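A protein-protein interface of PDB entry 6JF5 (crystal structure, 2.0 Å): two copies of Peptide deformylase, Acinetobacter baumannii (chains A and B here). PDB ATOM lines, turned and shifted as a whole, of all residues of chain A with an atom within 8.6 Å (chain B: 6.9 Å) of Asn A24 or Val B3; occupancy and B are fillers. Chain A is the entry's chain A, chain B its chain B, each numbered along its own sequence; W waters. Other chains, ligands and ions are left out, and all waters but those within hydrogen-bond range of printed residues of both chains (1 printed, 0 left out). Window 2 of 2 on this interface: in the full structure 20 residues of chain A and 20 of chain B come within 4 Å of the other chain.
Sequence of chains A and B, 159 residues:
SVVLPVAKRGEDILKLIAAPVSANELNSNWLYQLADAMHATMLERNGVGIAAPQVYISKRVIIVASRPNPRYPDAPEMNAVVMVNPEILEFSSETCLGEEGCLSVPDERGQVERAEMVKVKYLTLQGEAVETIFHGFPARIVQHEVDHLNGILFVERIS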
ATOM      1  N   VAL A  21      36.689  -6.905 -19.070  1.00  0.00           N
ATOM      2  CA  VAL A  21      35.493  -7.423 -19.770  1.00  0.00           C
ATOM      3  C   VAL A  21      34.709  -8.322 -18.807  1.00  0.00           C
ATOM      4  O   VAL A  21      35.355  -9.114 -18.090  1.00  0.00           O
ATOM      5  CB  VAL A  21      35.938  -8.154 -21.037  1.00  0.00           C
ATOM      6  CG1 VAL A  21      34.803  -8.860 -21.735  1.00  0.00           C
ATOM      7  CG2 VAL A  21      36.637  -7.184 -21.967  1.00  0.00           C
ATOM      8  N   SER A  22      33.375  -8.185 -18.770  1.00  0.00           N
ATOM      9  CA  SER A  22      32.477  -8.963 -17.869  1.00  0.00           C
ATOM     10  C   SER A  22      32.138 -10.329 -18.491  1.00  0.00           C
ATOM     11  O   SER A  22      32.241 -10.495 -19.719  1.00  0.00           O
ATOM     12  CB  SER A  22      31.227  -8.193 -17.583  1.00  0.00           C
ATOM     13  OG  SER A  22      30.433  -8.171 -18.756  1.00  0.00           O
ATOM     14  N   ALA A  23      31.720 -11.291 -17.674  1.00  0.00           N
ATOM     15  CA  ALA A  23      31.313 -12.623 -18.162  1.00  0.00           C
ATOM     16  C   ALA A  23      30.172 -12.452 -19.178  1.00  0.00           C
ATOM     17  O   ALA A  23      30.196 -13.153 -20.197  1.00  0.00           O
ATOM     18  CB  ALA A  23      30.960 -13.528 -17.002  1.00  0.00           C
ATOM     19  N   ASN A  24      29.278 -11.482 -18.978  1.00  0.00           N
ATOM     20  CA  ASN A  24      28.125 -11.199 -19.888  1.00  0.00           C
ATOM     21  C   ASN A  24      28.610 -11.046 -21.324  1.00  0.00           C
ATOM     22  O   ASN A  24      27.929 -11.507 -22.243  1.00  0.00           O
ATOM     23  CB  ASN A  24      27.383  -9.918 -19.510  1.00  0.00           C
ATOM     24  CG  ASN A  24      26.411 -10.122 -18.374  1.00  0.00           C
ATOM     25  OD1 ASN A  24      25.203 -10.195 -18.591  1.00  0.00           O
ATOM     26  ND2 ASN A  24      26.920 -10.193 -17.167  1.00  0.00           N
ATOM     27  N   GLU A  25      29.766 -10.417 -21.519  1.00  0.00           N
ATOM     28  CA  GLU A  25      30.248 -10.004 -22.866  1.00  0.00           C
ATOM     29  C   GLU A  25      30.903 -11.193 -23.580  1.00  0.00           C
ATOM     30  O   GLU A  25      31.035 -11.165 -24.809  1.00  0.00           O
ATOM     31  CB  GLU A  25      31.252  -8.847 -22.732  1.00  0.00           C
ATOM     32  CG  GLU A  25      30.683  -7.568 -22.161  1.00  0.00           C
ATOM     33  CD  GLU A  25      31.751  -6.531 -21.809  1.00  0.00           C
ATOM     34  OE1 GLU A  25      32.103  -6.394 -20.605  1.00  0.00           O
ATOM     35  OE2 GLU A  25      32.283  -5.905 -22.764  1.00  0.00           O
ATOM     36  N   LEU A  26      31.388 -12.185 -22.852  1.00  0.00           N
ATOM     37  CA  LEU A  26      32.089 -13.339 -23.482  1.00  0.00           C
ATOM     38  C   LEU A  26      31.147 -14.088 -24.442  1.00  0.00           C
ATOM     39  O   LEU A  26      29.967 -14.238 -24.118  1.00  0.00           O
ATOM     40  CB  LEU A  26      32.627 -14.248 -22.384  1.00  0.00           C
ATOM     41  CG  LEU A  26      33.598 -13.568 -21.426  1.00  0.00           C
ATOM     42  CD1 LEU A  26      33.907 -14.500 -20.248  1.00  0.00           C
ATOM     43  CD2 LEU A  26      34.850 -13.092 -22.171  1.00  0.00           C
ATOM     44  N   ASN A  27      31.643 -14.432 -25.624  1.00  0.00           N
ATOM     45  CA  ASN A  27      30.903 -15.226 -26.643  1.00  0.00           C
ATOM     46  C   ASN A  27      29.710 -14.409 -27.185  1.00  0.00           C
ATOM     47  O   ASN A  27      28.686 -15.001 -27.586  1.00  0.00           O
ATOM     48  CB  ASN A  27      30.495 -16.549 -26.014  1.00  0.00           C
ATOM     49  CG  ASN A  27      30.079 -17.606 -27.006  1.00  0.00           C
ATOM     50  OD1 ASN A  27      29.130 -18.324 -26.712  1.00  0.00           O
ATOM     51  ND2 ASN A  27      30.759 -17.716 -28.141  1.00  0.00           N
ATOM     52  N   SER A  28      29.818 -13.081 -27.197  1.00  0.00           N
ATOM     53  CA  SER A  28      28.717 -12.185 -27.626  1.00  0.00           C
ATOM     54  C   SER A  28      29.056 -11.641 -29.009  1.00  0.00           C
ATOM     55  O   SER A  28      30.265 -11.566 -29.353  1.00  0.00           O
ATOM     56  CB  SER A  28      28.445 -11.093 -26.643  1.00  0.00           C
ATOM     57  OG  SER A  28      29.537 -10.180 -26.542  1.00  0.00           O
ATOM     58  N   ASN A  29      28.019 -11.330 -29.785  1.00  0.00           N
ATOM     59  CA  ASN A  29      28.152 -10.560 -31.037  1.00  0.00           C
ATOM     60  C   ASN A  29      28.870  -9.246 -30.732  1.00  0.00           C
ATOM     61  O   ASN A  29      29.679  -8.823 -31.538  1.00  0.00           O
ATOM     62  CB  ASN A  29      26.796 -10.340 -31.707  1.00  0.00           C
ATOM     63  CG  ASN A  29      26.232 -11.611 -32.304  1.00  0.00           C
ATOM     64  OD1 ASN A  29      26.976 -12.428 -32.826  1.00  0.00           O
ATOM     65  ND2 ASN A  29      24.924 -11.792 -32.220  1.00  0.00           N
ATOM     66  N   TRP A  30      28.575  -8.611 -29.612  1.00  0.00           N
ATOM     67  CA  TRP A  30      29.205  -7.326 -29.229  1.00  0.00           C
ATOM     68  C   TRP A  30      30.729  -7.509 -29.213  1.00  0.00           C
ATOM     69  O   TRP A  30      31.453  -6.729 -29.836  1.00  0.00           O
ATOM     70  CB  TRP A  30      28.625  -6.833 -27.890  1.00  0.00           C
ATOM     71  CG  TRP A  30      29.593  -6.013 -27.095  1.00  0.00           C
ATOM     72  CD1 TRP A  30      30.145  -6.361 -25.900  1.00  0.00           C
ATOM     73  CD2 TRP A  30      30.155  -4.733 -27.434  1.00  0.00           C
ATOM     74  NE1 TRP A  30      31.014  -5.398 -25.471  1.00  0.00           N
ATOM     75  CE2 TRP A  30      31.045  -4.387 -26.389  1.00  0.00           C
ATOM     76  CE3 TRP A  30      30.013  -3.852 -28.512  1.00  0.00           C
ATOM     77  CZ2 TRP A  30      31.776  -3.196 -26.389  1.00  0.00           C
ATOM     78  CZ3 TRP A  30      30.740  -2.683 -28.522  1.00  0.00           C
ATOM     79  CH2 TRP A  30      31.616  -2.362 -27.477  1.00  0.00           C
ATOM     80  N   LEU A  31      31.215  -8.570 -28.590  1.00  0.00           N
ATOM     81  CA  LEU A  31      32.667  -8.715 -28.318  1.00  0.00           C
ATOM     82  C   LEU A  31      33.378  -9.101 -29.608  1.00  0.00           C
ATOM     83  O   LEU A  31      34.451  -8.587 -29.840  1.00  0.00           O
ATOM     84  CB  LEU A  31      32.892  -9.744 -27.212  1.00  0.00           C
ATOM     85  CG  LEU A  31      34.329  -9.847 -26.712  1.00  0.00           C
ATOM     86  CD1 LEU A  31      34.818  -8.495 -26.214  1.00  0.00           C
ATOM     87  CD2 LEU A  31      34.463 -10.906 -25.612  1.00  0.00           C
ATOM     88  N   LYS A  59      38.319  -0.866 -22.013  1.00  0.00           N
ATOM     89  CA  LYS A  59      38.128  -2.319 -21.752  1.00  0.00           C
ATOM     90  C   LYS A  59      39.461  -3.054 -21.954  1.00  0.00           C
ATOM     91  O   LYS A  59      40.267  -2.596 -22.757  1.00  0.00           O
ATOM     92  CB  LYS A  59      36.999  -2.866 -22.641  1.00  0.00           C
ATOM     93  CG  LYS A  59      35.607  -2.429 -22.195  1.00  0.00           C
ATOM     94  CD  LYS A  59      34.493  -3.050 -22.976  1.00  0.00           C
ATOM     95  CE  LYS A  59      33.128  -2.865 -22.346  1.00  0.00           C
ATOM     96  NZ  LYS A  59      32.983  -3.672 -21.102  1.00  0.00           N
ATOM     97  N   LEU A 125      37.743 -14.999 -27.038  1.00  0.00           N
ATOM     98  CA  LEU A 125      36.468 -14.286 -27.314  1.00  0.00           C
ATOM     99  C   LEU A 125      35.275 -15.134 -26.875  1.00  0.00           C
ATOM    100  O   LEU A 125      34.248 -14.531 -26.516  1.00  0.00           O
ATOM    101  CB  LEU A 125      36.395 -13.985 -28.811  1.00  0.00           C
ATOM    102  CG  LEU A 125      37.405 -12.945 -29.269  1.00  0.00           C
ATOM    103  CD1 LEU A 125      37.420 -12.836 -30.788  1.00  0.00           C
ATOM    104  CD2 LEU A 125      37.091 -11.604 -28.612  1.00  0.00           C
ATOM    105  N   SER B   1      21.364 -10.342 -27.014  1.00  0.00           N
ATOM    106  CA  SER B   1      21.652  -8.976 -26.454  1.00  0.00           C
ATOM    107  C   SER B   1      22.443  -9.092 -25.148  1.00  0.00           C
ATOM    108  O   SER B   1      22.022  -9.857 -24.277  1.00  0.00           O
ATOM    109  CB  SER B   1      20.387  -8.222 -26.240  1.00  0.00           C
ATOM    110  OG  SER B   1      19.666  -8.106 -27.454  1.00  0.00           O
ATOM    111  N   VAL B   2      23.544  -8.348 -25.027  1.00  0.00           N
ATOM    112  CA  VAL B   2      24.492  -8.352 -23.873  1.00  0.00           C
ATOM    113  C   VAL B   2      24.154  -7.204 -22.920  1.00  0.00           C
ATOM    114  O   VAL B   2      24.000  -6.076 -23.403  1.00  0.00           O
ATOM    115  CB  VAL B   2      25.932  -8.206 -24.409  1.00  0.00           C
ATOM    116  CG1 VAL B   2      26.952  -7.901 -23.332  1.00  0.00           C
ATOM    117  CG2 VAL B   2      26.346  -9.415 -25.201  1.00  0.00           C
ATOM    118  N   VAL B   3      24.131  -7.455 -21.619  1.00  0.00           N
ATOM    119  CA  VAL B   3      24.083  -6.399 -20.564  1.00  0.00           C
ATOM    120  C   VAL B   3      25.528  -6.068 -20.200  1.00  0.00           C
ATOM    121  O   VAL B   3      26.265  -6.995 -19.865  1.00  0.00           O
ATOM    122  CB  VAL B   3      23.294  -6.872 -19.326  1.00  0.00           C
ATOM    123  CG1 VAL B   3      23.360  -5.876 -18.181  1.00  0.00           C
ATOM    124  CG2 VAL B   3      21.858  -7.164 -19.677  1.00  0.00           C
ATOM    125  N   LEU B   4      25.945  -4.814 -20.334  1.00  0.00           N
ATOM    126  CA  LEU B   4      27.372  -4.425 -20.154  1.00  0.00           C
ATOM    127  C   LEU B   4      27.587  -3.947 -18.726  1.00  0.00           C
ATOM    128  O   LEU B   4      26.649  -3.449 -18.110  1.00  0.00           O
ATOM    129  CB  LEU B   4      27.690  -3.285 -21.124  1.00  0.00           C
ATOM    130  CG  LEU B   4      27.635  -3.612 -22.616  1.00  0.00           C
ATOM    131  CD1 LEU B   4      27.794  -2.331 -23.443  1.00  0.00           C
ATOM    132  CD2 LEU B   4      28.711  -4.610 -22.961  1.00  0.00           C
ATOM    133  N   PRO B   5      28.815  -4.039 -18.177  1.00  0.00           N
ATOM    134  CA  PRO B   5      29.142  -3.370 -16.922  1.00  0.00           C
ATOM    135  C   PRO B   5      29.039  -1.834 -17.001  1.00  0.00           C
ATOM    136  O   PRO B   5      29.352  -1.227 -18.041  1.00  0.00           O
ATOM    137  CB  PRO B   5      30.604  -3.742 -16.638  1.00  0.00           C
ATOM    138  CG  PRO B   5      31.152  -4.227 -17.962  1.00  0.00           C
ATOM    139  CD  PRO B   5      29.958  -4.758 -18.743  1.00  0.00           C
ATOM    140  N   VAL B   6      28.560  -1.242 -15.914  1.00  0.00           N
ATOM    141  CA  VAL B   6      28.260   0.212 -15.800  1.00  0.00           C
ATOM    142  C   VAL B   6      29.276   0.856 -14.860  1.00  0.00           C
ATOM    143  O   VAL B   6      29.501   0.307 -13.747  1.00  0.00           O
ATOM    144  CB  VAL B   6      26.818   0.400 -15.342  1.00  0.00           C
ATOM    145  CG1 VAL B   6      26.493   1.845 -14.973  1.00  0.00           C
ATOM    146  CG2 VAL B   6      25.874  -0.111 -16.419  1.00  0.00           C
ATOM    147  N   ALA B  37      23.682  -3.386 -27.263  1.00  0.00           N
ATOM    148  CA  ALA B  37      24.251  -3.701 -25.927  1.00  0.00           C
ATOM    149  C   ALA B  37      23.937  -2.554 -24.939  1.00  0.00           C
ATOM    150  O   ALA B  37      23.475  -2.838 -23.808  1.00  0.00           O
ATOM    151  CB  ALA B  37      25.711  -3.978 -26.057  1.00  0.00           C
ATOM    152  N   ALA B  40      20.111  -2.968 -24.108  1.00  0.00           N
ATOM    153  CA  ALA B  40      19.916  -4.120 -23.191  1.00  0.00           C
ATOM    154  C   ALA B  40      20.390  -3.707 -21.800  1.00  0.00           C
ATOM    155  O   ALA B  40      19.694  -4.010 -20.809  1.00  0.00           O
ATOM    156  CB  ALA B  40      20.622  -5.362 -23.687  1.00  0.00           C
ATOM    157  N   THR B  41      21.484  -2.948 -21.713  1.00  0.00           N
ATOM    158  CA  THR B  41      21.991  -2.479 -20.397  1.00  0.00           C
ATOM    159  C   THR B  41      20.954  -1.548 -19.759  1.00  0.00           C
ATOM    160  O   THR B  41      20.682  -1.707 -18.564  1.00  0.00           O
ATOM    161  CB  THR B  41      23.375  -1.827 -20.500  1.00  0.00           C
ATOM    162  OG1 THR B  41      24.202  -2.784 -21.152  1.00  0.00           O
ATOM    163  CG2 THR B  41      23.944  -1.454 -19.142  1.00  0.00           C
ATOM    164  N   MET B  42      20.454  -0.554 -20.501  1.00  0.00           N
ATOM    165  CA  MET B  42      19.481   0.418 -19.940  1.00  0.00           C
ATOM    166  C   MET B  42      18.242  -0.364 -19.424  1.00  0.00           C
ATOM    167  O   MET B  42      17.805  -0.118 -18.297  1.00  0.00           O
ATOM    168  CB  MET B  42      19.112   1.425 -21.019  1.00  0.00           C
ATOM    169  CG  MET B  42      18.143   2.496 -20.636  1.00  0.00           C
ATOM    170  SD  MET B  42      17.471   3.251 -22.152  1.00  0.00           S
ATOM    171  CE  MET B  42      16.142   2.122 -22.560  1.00  0.00           C
ATOM    172  N   LEU B  43      17.670  -1.264 -20.214  1.00  0.00           N
ATOM    173  CA  LEU B  43      16.455  -2.028 -19.796  1.00  0.00           C
ATOM    174  C   LEU B  43      16.755  -2.876 -18.545  1.00  0.00           C
ATOM    175  O   LEU B  43      15.957  -2.828 -17.636  1.00  0.00           O
ATOM    176  CB  LEU B  43      15.974  -2.888 -20.961  1.00  0.00           C
ATOM    177  CG  LEU B  43      15.395  -2.113 -22.135  1.00  0.00           C
ATOM    178  CD1 LEU B  43      14.957  -3.057 -23.250  1.00  0.00           C
ATOM    179  CD2 LEU B  43      14.234  -1.228 -21.701  1.00  0.00           C
ATOM    180  N   GLU B  44      17.890  -3.571 -18.475  1.00  0.00           N
ATOM    181  CA  GLU B  44      18.270  -4.444 -17.327  1.00  0.00           C
ATOM    182  C   GLU B  44      18.274  -3.632 -16.036  1.00  0.00           C
ATOM    183  O   GLU B  44      18.011  -4.221 -14.988  1.00  0.00           O
ATOM    184  CB  GLU B  44      19.637  -5.085 -17.547  1.00  0.00           C
ATOM    185  CG  GLU B  44      20.490  -5.213 -16.285  1.00  0.00           C
ATOM    186  CD  GLU B  44      20.257  -6.476 -15.486  1.00  0.00           C
ATOM    187  OE1 GLU B  44      19.752  -7.461 -16.079  1.00  0.00           O
ATOM    188  OE2 GLU B  44      20.580  -6.475 -14.275  1.00  0.00           O
ATOM    189  N   ARG B  45      18.588  -2.333 -16.100  1.00  0.00           N
ATOM    190  CA  ARG B  45      18.666  -1.468 -14.900  1.00  0.00           C
ATOM    191  C   ARG B  45      17.378  -0.653 -14.756  1.00  0.00           C
ATOM    192  O   ARG B  45      17.321   0.216 -13.887  1.00  0.00           O
ATOM    193  CB  ARG B  45      19.890  -0.554 -15.007  1.00  0.00           C
ATOM    194  CG  ARG B  45      21.225  -1.277 -15.084  1.00  0.00           C
ATOM    195  CD  ARG B  45      21.548  -1.932 -13.750  1.00  0.00           C
ATOM    196  NE  ARG B  45      22.958  -2.272 -13.613  1.00  0.00           N
ATOM    197  CZ  ARG B  45      23.922  -1.427 -13.239  1.00  0.00           C
ATOM    198  NH1 ARG B  45      25.169  -1.857 -13.141  1.00  0.00           N
ATOM    199  NH2 ARG B  45      23.643  -0.164 -12.952  1.00  0.00           N
ATOM    200  N   VAL B  55      29.138   2.759 -20.021  1.00  0.00           N
ATOM    201  CA  VAL B  55      29.565   1.357 -20.285  1.00  0.00           C
ATOM    202  C   VAL B  55      31.011   1.315 -20.811  1.00  0.00           C
ATOM    203  O   VAL B  55      31.363   0.355 -21.526  1.00  0.00           O
ATOM    204  CB  VAL B  55      28.532   0.664 -21.186  1.00  0.00           C
ATOM    205  CG1 VAL B  55      27.169   0.585 -20.485  1.00  0.00           C
ATOM    206  CG2 VAL B  55      28.361   1.337 -22.524  1.00  0.00           C
HETATM  207  O   HOH W   1      30.858  -1.934 -20.309  1.00  0.00           O
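Of the printed residues of chain B, Ser A22 touches Pro B5. Printed residues of chain B within 4 Å of Asn A24: Val B2 (3.9 Å) and Val B3 (3.1 Å). Printed residues of chain B within 4 Å of Glu A25: Val B2, Leu B4 and Pro B5. Of the printed residues of chain B, Lys A59 touches Pro B5 and Val B55. Of chain A, only Asn A24, Glu A25 and Ser A28 come within 4 Å of Val B2. Of the printed residues of chain A, Val B3 touches Asn A24 (3.1 Å). Of the printed residues of chain A, Leu B4 touches Glu A25 (3.6 Å) and Trp A30 (3.5 Å). Of the printed residues of chain A, Val B55 touches Lys A59 (3.8 Å). The nearest residue of chain A that does not touch Val B3 is Ser A22 (4.5 Å). The nearest printed residue of chain B that does not touch Ser A28 is Ser B1 (6.5 Å).
N of Leu B4 sits at hydrogen-bond distance from OG1 of Thr B41 (2.8 Å). The backbone NH (N) of Ser A22 sits at hydrogen-bond distance from the side-chain carboxylate (OE1) of Glu A25 (2.9 Å). OG of Ser A28 is in hydrogen-bond range of O of Glu A25, at 2.5 Å. The side-chain carboxylate (OE2) of Glu A25 is in hydrogen-bond range of the indole nitrogen (NE1) of Trp A30, 3.0 Å away. NZ of Lys A59 lies within salt-bridge range of OE2 of Glu A25, at 2.9 Å. OG of Ser A28 lies within hydrogen-bond range of N of Leu A31, at 3.1 Å.
No position is printed for both chains. Of the 10 pairs that touch across the chains among the printed residues, none has its exchanged pair printed and touching as well.
OG of Ser A22 touches CD of Pro B5, 3.4 Å away. O of Asn A24 touches CG1 of Val B2, 3.9 Å away. Asn A24 touches Val B3. Glu A25 touches Val B2 (CG to CG1, 3.9 Å). CG of Glu A25 touches CD2 of Leu B4, at 3.6 Å. CD of Pro B5 touches OE1 of Glu A25, at 3.3 Å. Ser A28 touches Val B2 (CB to CG2, 3.0 Å). Leu B4 touches Trp A30. CG of Pro B5 touches NZ of Lys A59 (3.7 Å). Val B55 touches Lys A59 (O to CE, 3.8 Å).
Water W1 lies within hydrogen-bond range of the backbone carbonyl oxygen (O) of Val B55 (2.6 Å), the backbone carbonyl oxygen (O) of Pro B5 (2.8 Å) and the side-chain amino group (NZ) of Lys A59 (2.9 Å).
Of the 13 printed residues of chain A, 6 touch a printed residue of chain B. Of the 14 printed residues of chain B, 5 touch a printed residue of chain A. Hydrophobic or aromatic side chains of chain B within 4 Å of the printed part of chain A: Val B2, Val B3, Leu B4 and Pro B5. Among the printed residues, 10 pairs touch across the chains. Among the printed residues, no Asp or Glu carboxylate lies within 4 Å of a Lys or Arg side-chain nitrogen of the other chain.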
